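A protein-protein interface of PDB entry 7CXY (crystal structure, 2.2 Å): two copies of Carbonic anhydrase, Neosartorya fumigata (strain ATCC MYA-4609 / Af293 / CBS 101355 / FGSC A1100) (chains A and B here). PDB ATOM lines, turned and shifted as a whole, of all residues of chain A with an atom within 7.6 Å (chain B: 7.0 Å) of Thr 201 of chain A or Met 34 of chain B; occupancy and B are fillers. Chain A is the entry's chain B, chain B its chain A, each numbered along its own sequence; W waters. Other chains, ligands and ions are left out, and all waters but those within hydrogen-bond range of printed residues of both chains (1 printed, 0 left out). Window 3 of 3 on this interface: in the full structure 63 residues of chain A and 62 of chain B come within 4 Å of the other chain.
The side-chain amide nitrogen (ND2) of Asn 26 of chain B is in hydrogen-bond range of the backbone carbonyl oxygen (O) of Gly 202 of chain A, 3.1 Å away. The side-chain amide oxygen (OD1) of Asn 26 of chain B is in hydrogen-bond range of the backbone NH (N) of Leu 204 of chain A, at 2.9 Å. OE2 of Glu 200 of chain A is in hydrogen-bond range of OG of Ser 45 of chain B, at 3.1 Å. The backbone carbonyl oxygen (O) of Val 199 of chain A sits close to the backbone carbonyl oxygen (O) of Phe 41 of chain B (3.4 Å).
No position is printed for both chains. Of the 14 pairs that touch across the chains among the printed residues, none has its exchanged pair printed and touching as well.
Of the 17 printed residues of chain B, 6 touch a printed residue of chain A. Printed residues of chain B that touch a printed residue of chain A: Asn 26, Trp 29, Val 30, Met 34, Phe 41 and Ser 45. Hydrophobic or aromatic side chains of chain B that line the printed part of chain A: Trp 29, Val 30, Met 34 and Phe 41. Among the printed residues, 14 pairs touch across the chains.
Water W1 lies within hydrogen-bond range of OD1 of Asn 26 of chain B and O of Leu 204 of chain A.
O of Phe 41 of chain B is in hydrogen-bond range of OG of Ser 45 of chain B (2.8 Å). O of Glu 42 of chain B sits at hydrogen-bond distance from OG of Ser 45 of chain B, at 3.3 Å. OD1 of Asp 198 of chain A sits at hydrogen-bond distance from N of Glu 200 of chain A (3.2 Å). The backbone carbonyl oxygen (O) of Asp 198 of chain A sits at hydrogen-bond distance from the side-chain hydroxyl (OG1) of Thr 201 of chain A (3.4 Å). The backbone carbonyl oxygen of Leu 203 of chain A lies within hydrogen-bond range of the backbone NH of Asp 198 of chain A. The backbone NH (N) of Leu 203 of chain A sits at hydrogen-bond distance from the side-chain hydroxyl (OG1) of Thr 201 of chain A (3.0 Å).
Among the printed residues, pairs that only touch across the chains: Glu 200 of chain A with Phe 41 of chain B (3.1 Å), Gly 202 of chain A with Val 30 of chain B (3.2 Å), Thr 201 of chain A with Val 30 of chain B (3.4 Å), Leu 203 of chain A with Asn 26 of chain B (3.4 Å), Gly 202 of chain A with Trp 29 of chain B (3.5 Å), Gly 202 of chain A with Phe 41 of chain B (3.6 Å), Thr 201 of chain A with Phe 41 of chain B (3.7 Å), Leu 203 of chain A with Val 30 of chain B (3.9 Å), Val 199 of chain A with Ser 45 of chain B (3.9 Å) and Thr 201 of chain A with Met 34 of chain B (3.9 Å).
Printed residues of chain B within 4 Å of Val 199 of chain A: Phe 41 (3.3 Å) and Ser 45 (3.9 Å). Of the printed residues of chain B, Glu 200 of chain A touches Phe 41 (3.1 Å) and Ser 45 (3.1 Å). Thr 201 of chain A touches three residues of chain B. Of the printed residues of chain B, Leu 203 of chain A touches Asn 26 and Val 30. Printed residues of chain A within 4 Å of Asn 26 of chain B: Gly 202, Leu 203 and Leu 204. Ala 28 of chain B touches none of the printed residues of chain A. Met 34 of chain B touches just one residue of chain A: Thr 201 (3.9 Å). Of the printed residues of chain A, Phe 41 of chain B touches Val 199, Glu 200, Thr 201 and Gly 202. Glu 42 of chain B touches none of the printed residues of chain A. The nearest residue of chain A that does not touch Met 34 of chain B is Glu 200 of chain A (5.7 Å). The nearest printed residue of chain A that does not touch Phe 41 of chain B is Phe 197 of chain A (5.2 Å).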
ATOM      1  N   PHE A 197      31.541 -31.067 -19.652  1.00  0.00           N
ATOM      2  CA  PHE A 197      30.387 -30.742 -18.790  1.00  0.00           C
ATOM      3  C   PHE A 197      29.354 -30.040 -19.667  1.00  0.00           C
ATOM      4  O   PHE A 197      29.700 -29.126 -20.387  1.00  0.00           O
ATOM      5  CB  PHE A 197      30.794 -29.913 -17.574  1.00  0.00           C
ATOM      6  CG  PHE A 197      29.626 -29.349 -16.806  1.00  0.00           C
ATOM      7  CD1 PHE A 197      28.814 -30.169 -16.048  1.00  0.00           C
ATOM      8  CD2 PHE A 197      29.313 -28.006 -16.872  1.00  0.00           C
ATOM      9  CE1 PHE A 197      27.734 -29.662 -15.352  1.00  0.00           C
ATOM     10  CE2 PHE A 197      28.233 -27.497 -16.175  1.00  0.00           C
ATOM     11  CZ  PHE A 197      27.454 -28.325 -15.409  1.00  0.00           C
ATOM     12  N   ASP A 198      28.115 -30.505 -19.637  1.00  0.00           N
ATOM     13  CA  ASP A 198      27.073 -29.854 -20.468  1.00  0.00           C
ATOM     14  C   ASP A 198      26.147 -29.056 -19.559  1.00  0.00           C
ATOM     15  O   ASP A 198      25.410 -29.676 -18.834  1.00  0.00           O
ATOM     16  CB  ASP A 198      26.284 -30.904 -21.244  1.00  0.00           C
ATOM     17  CG  ASP A 198      25.327 -30.354 -22.277  1.00  0.00           C
ATOM     18  OD1 ASP A 198      25.215 -29.148 -22.405  1.00  0.00           O
ATOM     19  OD2 ASP A 198      24.716 -31.158 -22.939  1.00  0.00           O
ATOM     20  N   VAL A 199      26.153 -27.731 -19.675  1.00  0.00           N
ATOM     21  CA  VAL A 199      25.294 -26.845 -18.833  1.00  0.00           C
ATOM     22  C   VAL A 199      23.813 -27.076 -19.112  1.00  0.00           C
ATOM     23  O   VAL A 199      23.030 -26.841 -18.224  1.00  0.00           O
ATOM     24  CB  VAL A 199      25.603 -25.349 -18.958  1.00  0.00           C
ATOM     25  CG1 VAL A 199      26.372 -24.841 -17.771  1.00  0.00           C
ATOM     26  CG2 VAL A 199      26.225 -24.978 -20.282  1.00  0.00           C
ATOM     27  N   GLU A 200      23.452 -27.441 -20.335  1.00  0.00           N
ATOM     28  CA  GLU A 200      22.028 -27.653 -20.681  1.00  0.00           C
ATOM     29  C   GLU A 200      21.437 -28.765 -19.812  1.00  0.00           C
ATOM     30  O   GLU A 200      20.314 -28.608 -19.412  1.00  0.00           O
ATOM     31  CB  GLU A 200      21.886 -27.954 -22.167  1.00  0.00           C
ATOM     32  CG  GLU A 200      22.319 -26.812 -23.059  1.00  0.00           C
ATOM     33  CD  GLU A 200      21.345 -25.665 -23.234  1.00  0.00           C
ATOM     34  OE1 GLU A 200      20.138 -25.922 -23.321  1.00  0.00           O
ATOM     35  OE2 GLU A 200      21.797 -24.512 -23.300  1.00  0.00           O
ATOM     36  N   THR A 201      22.180 -29.829 -19.528  1.00  0.00           N
ATOM     37  CA  THR A 201      21.644 -30.951 -18.729  1.00  0.00           C
ATOM     38  C   THR A 201      22.345 -31.127 -17.389  1.00  0.00           C
ATOM     39  O   THR A 201      21.857 -31.921 -16.603  1.00  0.00           O
ATOM     40  CB  THR A 201      21.944 -32.249 -19.467  1.00  0.00           C
ATOM     41  OG1 THR A 201      23.360 -32.370 -19.476  1.00  0.00           O
ATOM     42  CG2 THR A 201      21.468 -32.197 -20.896  1.00  0.00           C
ATOM     43  N   GLY A 202      23.527 -30.539 -17.217  1.00  0.00           N
ATOM     44  CA  GLY A 202      24.322 -30.707 -15.987  1.00  0.00           C
ATOM     45  C   GLY A 202      25.066 -32.034 -15.938  1.00  0.00           C
ATOM     46  O   GLY A 202      25.674 -32.317 -14.933  1.00  0.00           O
ATOM     47  N   LEU A 203      25.075 -32.792 -17.027  1.00  0.00           N
ATOM     48  CA  LEU A 203      25.703 -34.131 -17.063  1.00  0.00           C
ATOM     49  C   LEU A 203      27.140 -34.085 -17.577  1.00  0.00           C
ATOM     50  O   LEU A 203      27.417 -33.357 -18.510  1.00  0.00           O
ATOM     51  CB  LEU A 203      24.861 -35.020 -17.975  1.00  0.00           C
ATOM     52  CG  LEU A 203      23.481 -35.386 -17.449  1.00  0.00           C
ATOM     53  CD1 LEU A 203      22.684 -36.070 -18.531  1.00  0.00           C
ATOM     54  CD2 LEU A 203      23.602 -36.285 -16.242  1.00  0.00           C
ATOM     55  N   LEU A 204      27.985 -34.892 -16.956  1.00  0.00           N
ATOM     56  CA  LEU A 204      29.376 -35.106 -17.383  1.00  0.00           C
ATOM     57  C   LEU A 204      29.358 -36.199 -18.447  1.00  0.00           C
ATOM     58  O   LEU A 204      28.658 -37.167 -18.261  1.00  0.00           O
ATOM     59  CB  LEU A 204      30.187 -35.600 -16.190  1.00  0.00           C
ATOM     60  CG  LEU A 204      30.656 -34.538 -15.213  1.00  0.00           C
ATOM     61  CD1 LEU A 204      31.356 -35.182 -14.049  1.00  0.00           C
ATOM     62  CD2 LEU A 204      31.569 -33.543 -15.892  1.00  0.00           C
ATOM     63  N   ASN B  26      27.266 -37.665 -10.229  1.00  0.00           N
ATOM     64  CA  ASN B  26      26.894 -36.541 -11.116  1.00  0.00           C
ATOM     65  C   ASN B  26      25.412 -36.691 -11.480  1.00  0.00           C
ATOM     66  O   ASN B  26      24.702 -35.670 -11.504  1.00  0.00           O
ATOM     67  CB  ASN B  26      27.862 -36.443 -12.301  1.00  0.00           C
ATOM     68  CG  ASN B  26      27.331 -35.521 -13.365  1.00  0.00           C
ATOM     69  OD1 ASN B  26      26.940 -35.980 -14.430  1.00  0.00           O
ATOM     70  ND2 ASN B  26      27.258 -34.234 -13.060  1.00  0.00           N
ATOM     71  N   ALA B  28      22.979 -38.413  -9.757  1.00  0.00           N
ATOM     72  CA  ALA B  28      22.254 -38.103  -8.501  1.00  0.00           C
ATOM     73  C   ALA B  28      22.141 -36.576  -8.343  1.00  0.00           C
ATOM     74  O   ALA B  28      21.009 -36.069  -8.086  1.00  0.00           O
ATOM     75  CB  ALA B  28      22.959 -38.744  -7.328  1.00  0.00           C
ATOM     76  N   TRP B  29      23.258 -35.855  -8.525  1.00  0.00           N
ATOM     77  CA  TRP B  29      23.304 -34.374  -8.371  1.00  0.00           C
ATOM     78  C   TRP B  29      22.362 -33.708  -9.386  1.00  0.00           C
ATOM     79  O   TRP B  29      21.679 -32.744  -9.016  1.00  0.00           O
ATOM     80  CB  TRP B  29      24.741 -33.848  -8.480  1.00  0.00           C
ATOM     81  CG  TRP B  29      24.815 -32.357  -8.488  1.00  0.00           C
ATOM     82  CD1 TRP B  29      24.757 -31.536  -7.403  1.00  0.00           C
ATOM     83  CD2 TRP B  29      24.951 -31.503  -9.635  1.00  0.00           C
ATOM     84  NE1 TRP B  29      24.811 -30.226  -7.800  1.00  0.00           N
ATOM     85  CE2 TRP B  29      24.952 -30.172  -9.162  1.00  0.00           C
ATOM     86  CE3 TRP B  29      25.099 -31.723 -11.009  1.00  0.00           C
ATOM     87  CZ2 TRP B  29      25.097 -29.077 -10.010  1.00  0.00           C
ATOM     88  CZ3 TRP B  29      25.216 -30.638 -11.855  1.00  0.00           C
ATOM     89  CH2 TRP B  29      25.235 -29.334 -11.359  1.00  0.00           C
ATOM     90  N   VAL B  30      22.328 -34.199 -10.625  1.00  0.00           N
ATOM     91  CA  VAL B  30      21.420 -33.657 -11.677  1.00  0.00           C
ATOM     92  C   VAL B  30      19.959 -33.940 -11.281  1.00  0.00           C
ATOM     93  O   VAL B  30      19.109 -33.020 -11.501  1.00  0.00           O
ATOM     94  CB  VAL B  30      21.777 -34.182 -13.083  1.00  0.00           C
ATOM     95  CG1 VAL B  30      20.663 -33.954 -14.099  1.00  0.00           C
ATOM     96  CG2 VAL B  30      23.066 -33.535 -13.588  1.00  0.00           C
ATOM     97  N   ALA B  31      19.661 -35.130 -10.739  1.00  0.00           N
ATOM     98  CA  ALA B  31      18.291 -35.531 -10.307  1.00  0.00           C
ATOM     99  C   ALA B  31      17.767 -34.527  -9.269  1.00  0.00           C
ATOM    100  O   ALA B  31      16.713 -33.914  -9.499  1.00  0.00           O
ATOM    101  CB  ALA B  31      18.285 -36.941  -9.759  1.00  0.00           C
ATOM    102  N   THR B  32      18.513 -34.355  -8.179  1.00  0.00           N
ATOM    103  CA  THR B  32      18.279 -33.362  -7.099  1.00  0.00           C
ATOM    104  C   THR B  32      17.926 -31.988  -7.674  1.00  0.00           C
ATOM    105  O   THR B  32      16.912 -31.428  -7.257  1.00  0.00           O
ATOM    106  CB  THR B  32      19.524 -33.276  -6.215  1.00  0.00           C
ATOM    107  OG1 THR B  32      19.735 -34.621  -5.784  1.00  0.00           O
ATOM    108  CG2 THR B  32      19.389 -32.311  -5.058  1.00  0.00           C
ATOM    109  N   LYS B  33      18.739 -31.446  -8.575  1.00  0.00           N
ATOM    110  CA  LYS B  33      18.570 -30.050  -9.065  1.00  0.00           C
ATOM    111  C   LYS B  33      17.293 -29.950  -9.924  1.00  0.00           C
ATOM    112  O   LYS B  33      16.654 -28.872  -9.939  1.00  0.00           O
ATOM    113  CB  LYS B  33      19.848 -29.606  -9.782  1.00  0.00           C
ATOM    114  CG  LYS B  33      20.961 -29.108  -8.867  1.00  0.00           C
ATOM    115  CD  LYS B  33      20.712 -27.701  -8.341  1.00  0.00           C
ATOM    116  CE  LYS B  33      21.966 -26.914  -8.004  1.00  0.00           C
ATOM    117  NZ  LYS B  33      22.528 -27.260  -6.670  1.00  0.00           N
ATOM    118  N   MET B  34      16.905 -31.035 -10.601  1.00  0.00           N
ATOM    119  CA  MET B  34      15.667 -31.081 -11.427  1.00  0.00           C
ATOM    120  C   MET B  34      14.426 -31.186 -10.511  1.00  0.00           C
ATOM    121  O   MET B  34      13.402 -30.557 -10.859  1.00  0.00           O
ATOM    122  CB  MET B  34      15.726 -32.221 -12.450  1.00  0.00           C
ATOM    123  CG  MET B  34      16.637 -31.900 -13.644  1.00  0.00           C
ATOM    124  SD  MET B  34      16.902 -33.317 -14.763  1.00  0.00           S
ATOM    125  CE  MET B  34      18.040 -32.594 -15.950  1.00  0.00           C
ATOM    126  N   LYS B  35      14.493 -31.931  -9.388  1.00  0.00           N
ATOM    127  CA  LYS B  35      13.531 -31.845  -8.248  1.00  0.00           C
ATOM    128  C   LYS B  35      13.263 -30.370  -7.903  1.00  0.00           C
ATOM    129  O   LYS B  35      12.147 -29.902  -8.204  1.00  0.00           O
ATOM    130  CB  LYS B  35      14.042 -32.583  -7.005  1.00  0.00           C
ATOM    131  CG  LYS B  35      13.602 -34.035  -6.857  1.00  0.00           C
ATOM    132  CD  LYS B  35      13.544 -34.501  -5.408  1.00  0.00           C
ATOM    133  CE  LYS B  35      13.243 -35.977  -5.270  1.00  0.00           C
ATOM    134  NZ  LYS B  35      11.885 -36.316  -5.765  1.00  0.00           N
ATOM    135  N   ASP B  36      14.243 -29.669  -7.317  1.00  0.00           N
ATOM    136  CA  ASP B  36      14.152 -28.239  -6.902  1.00  0.00           C
ATOM    137  C   ASP B  36      13.501 -27.385  -8.002  1.00  0.00           C
ATOM    138  O   ASP B  36      12.467 -26.742  -7.714  1.00  0.00           O
ATOM    139  CB  ASP B  36      15.526 -27.653  -6.568  1.00  0.00           C
ATOM    140  CG  ASP B  36      16.178 -28.261  -5.340  1.00  0.00           C
ATOM    141  OD1 ASP B  36      15.913 -29.456  -5.070  1.00  0.00           O
ATOM    142  OD2 ASP B  36      16.946 -27.539  -4.671  1.00  0.00           O
ATOM    143  N   ASP B  37      14.098 -27.357  -9.199  1.00  0.00           N
ATOM    144  CA  ASP B  37      13.627 -26.527 -10.344  1.00  0.00           C
ATOM    145  C   ASP B  37      13.760 -27.338 -11.629  1.00  0.00           C
ATOM    146  O   ASP B  37      14.874 -27.579 -12.076  1.00  0.00           O
ATOM    147  CB  ASP B  37      14.399 -25.203 -10.428  1.00  0.00           C
ATOM    148  CG  ASP B  37      13.858 -24.215 -11.451  1.00  0.00           C
ATOM    149  OD1 ASP B  37      12.887 -24.563 -12.162  1.00  0.00           O
ATOM    150  OD2 ASP B  37      14.413 -23.094 -11.527  1.00  0.00           O
ATOM    151  N   PRO B  38      12.638 -27.745 -12.281  1.00  0.00           N
ATOM    152  CA  PRO B  38      12.665 -28.407 -13.591  1.00  0.00           C
ATOM    153  C   PRO B  38      13.483 -27.711 -14.691  1.00  0.00           C
ATOM    154  O   PRO B  38      13.941 -28.409 -15.575  1.00  0.00           O
ATOM    155  CB  PRO B  38      11.191 -28.404 -14.042  1.00  0.00           C
ATOM    156  CG  PRO B  38      10.410 -28.387 -12.751  1.00  0.00           C
ATOM    157  CD  PRO B  38      11.261 -27.575 -11.794  1.00  0.00           C
ATOM    158  N   ALA B  39      13.674 -26.386 -14.605  1.00  0.00           N
ATOM    159  CA  ALA B  39      14.359 -25.545 -15.621  1.00  0.00           C
ATOM    160  C   ALA B  39      15.659 -24.930 -15.072  1.00  0.00           C
ATOM    161  O   ALA B  39      16.117 -23.925 -15.662  1.00  0.00           O
ATOM    162  CB  ALA B  39      13.409 -24.468 -16.088  1.00  0.00           C
ATOM    163  N   PHE B  40      16.248 -25.508 -14.014  1.00  0.00           N
ATOM    164  CA  PHE B  40      17.495 -25.019 -13.370  1.00  0.00           C
ATOM    165  C   PHE B  40      18.597 -24.843 -14.425  1.00  0.00           C
ATOM    166  O   PHE B  40      19.190 -23.747 -14.497  1.00  0.00           O
ATOM    167  CB  PHE B  40      17.986 -25.978 -12.281  1.00  0.00           C
ATOM    168  CG  PHE B  40      19.314 -25.593 -11.670  1.00  0.00           C
ATOM    169  CD1 PHE B  40      19.400 -24.572 -10.732  1.00  0.00           C
ATOM    170  CD2 PHE B  40      20.483 -26.244 -12.030  1.00  0.00           C
ATOM    171  CE1 PHE B  40      20.618 -24.211 -10.173  1.00  0.00           C
ATOM    172  CE2 PHE B  40      21.703 -25.870 -11.480  1.00  0.00           C
ATOM    173  CZ  PHE B  40      21.770 -24.847 -10.560  1.00  0.00           C
ATOM    174  N   PHE B  41      18.871 -25.894 -15.203  1.00  0.00           N
ATOM    175  CA  PHE B  41      19.968 -25.939 -16.205  1.00  0.00           C
ATOM    176  C   PHE B  41      19.628 -25.044 -17.408  1.00  0.00           C
ATOM    177  O   PHE B  41      20.539 -24.465 -18.027  1.00  0.00           O
ATOM    178  CB  PHE B  41      20.285 -27.393 -16.569  1.00  0.00           C
ATOM    179  CG  PHE B  41      20.836 -28.172 -15.399  1.00  0.00           C
ATOM    180  CD1 PHE B  41      22.068 -27.850 -14.850  1.00  0.00           C
ATOM    181  CD2 PHE B  41      20.108 -29.193 -14.807  1.00  0.00           C
ATOM    182  CE1 PHE B  41      22.567 -28.545 -13.758  1.00  0.00           C
ATOM    183  CE2 PHE B  41      20.619 -29.897 -13.722  1.00  0.00           C
ATOM    184  CZ  PHE B  41      21.842 -29.567 -13.196  1.00  0.00           C
ATOM    185  N   GLU B  42      18.345 -24.922 -17.730  1.00  0.00           N
ATOM    186  CA  GLU B  42      17.834 -24.014 -18.792  1.00  0.00           C
ATOM    187  C   GLU B  42      18.166 -22.569 -18.397  1.00  0.00           C
ATOM    188  O   GLU B  42      18.651 -21.816 -19.265  1.00  0.00           O
ATOM    189  CB  GLU B  42      16.337 -24.250 -18.970  1.00  0.00           C
ATOM    190  CG  GLU B  42      15.734 -23.545 -20.163  1.00  0.00           C
ATOM    191  CD  GLU B  42      14.315 -23.998 -20.469  1.00  0.00           C
ATOM    192  OE1 GLU B  42      13.980 -24.073 -21.668  1.00  0.00           O
ATOM    193  OE2 GLU B  42      13.541 -24.276 -19.511  1.00  0.00           O
ATOM    194  N   SER B  45      22.217 -21.934 -18.093  1.00  0.00           N
ATOM    195  CA  SER B  45      22.873 -21.854 -19.429  1.00  0.00           C
ATOM    196  C   SER B  45      22.405 -20.625 -20.229  1.00  0.00           C
ATOM    197  O   SER B  45      22.944 -20.417 -21.337  1.00  0.00           O
ATOM    198  CB  SER B  45      22.691 -23.134 -20.215  1.00  0.00           C
ATOM    199  OG  SER B  45      21.324 -23.411 -20.451  1.00  0.00           O
HETATM  200  O   HOH W   1      26.903 -38.146 -15.943  1.00  0.00           O
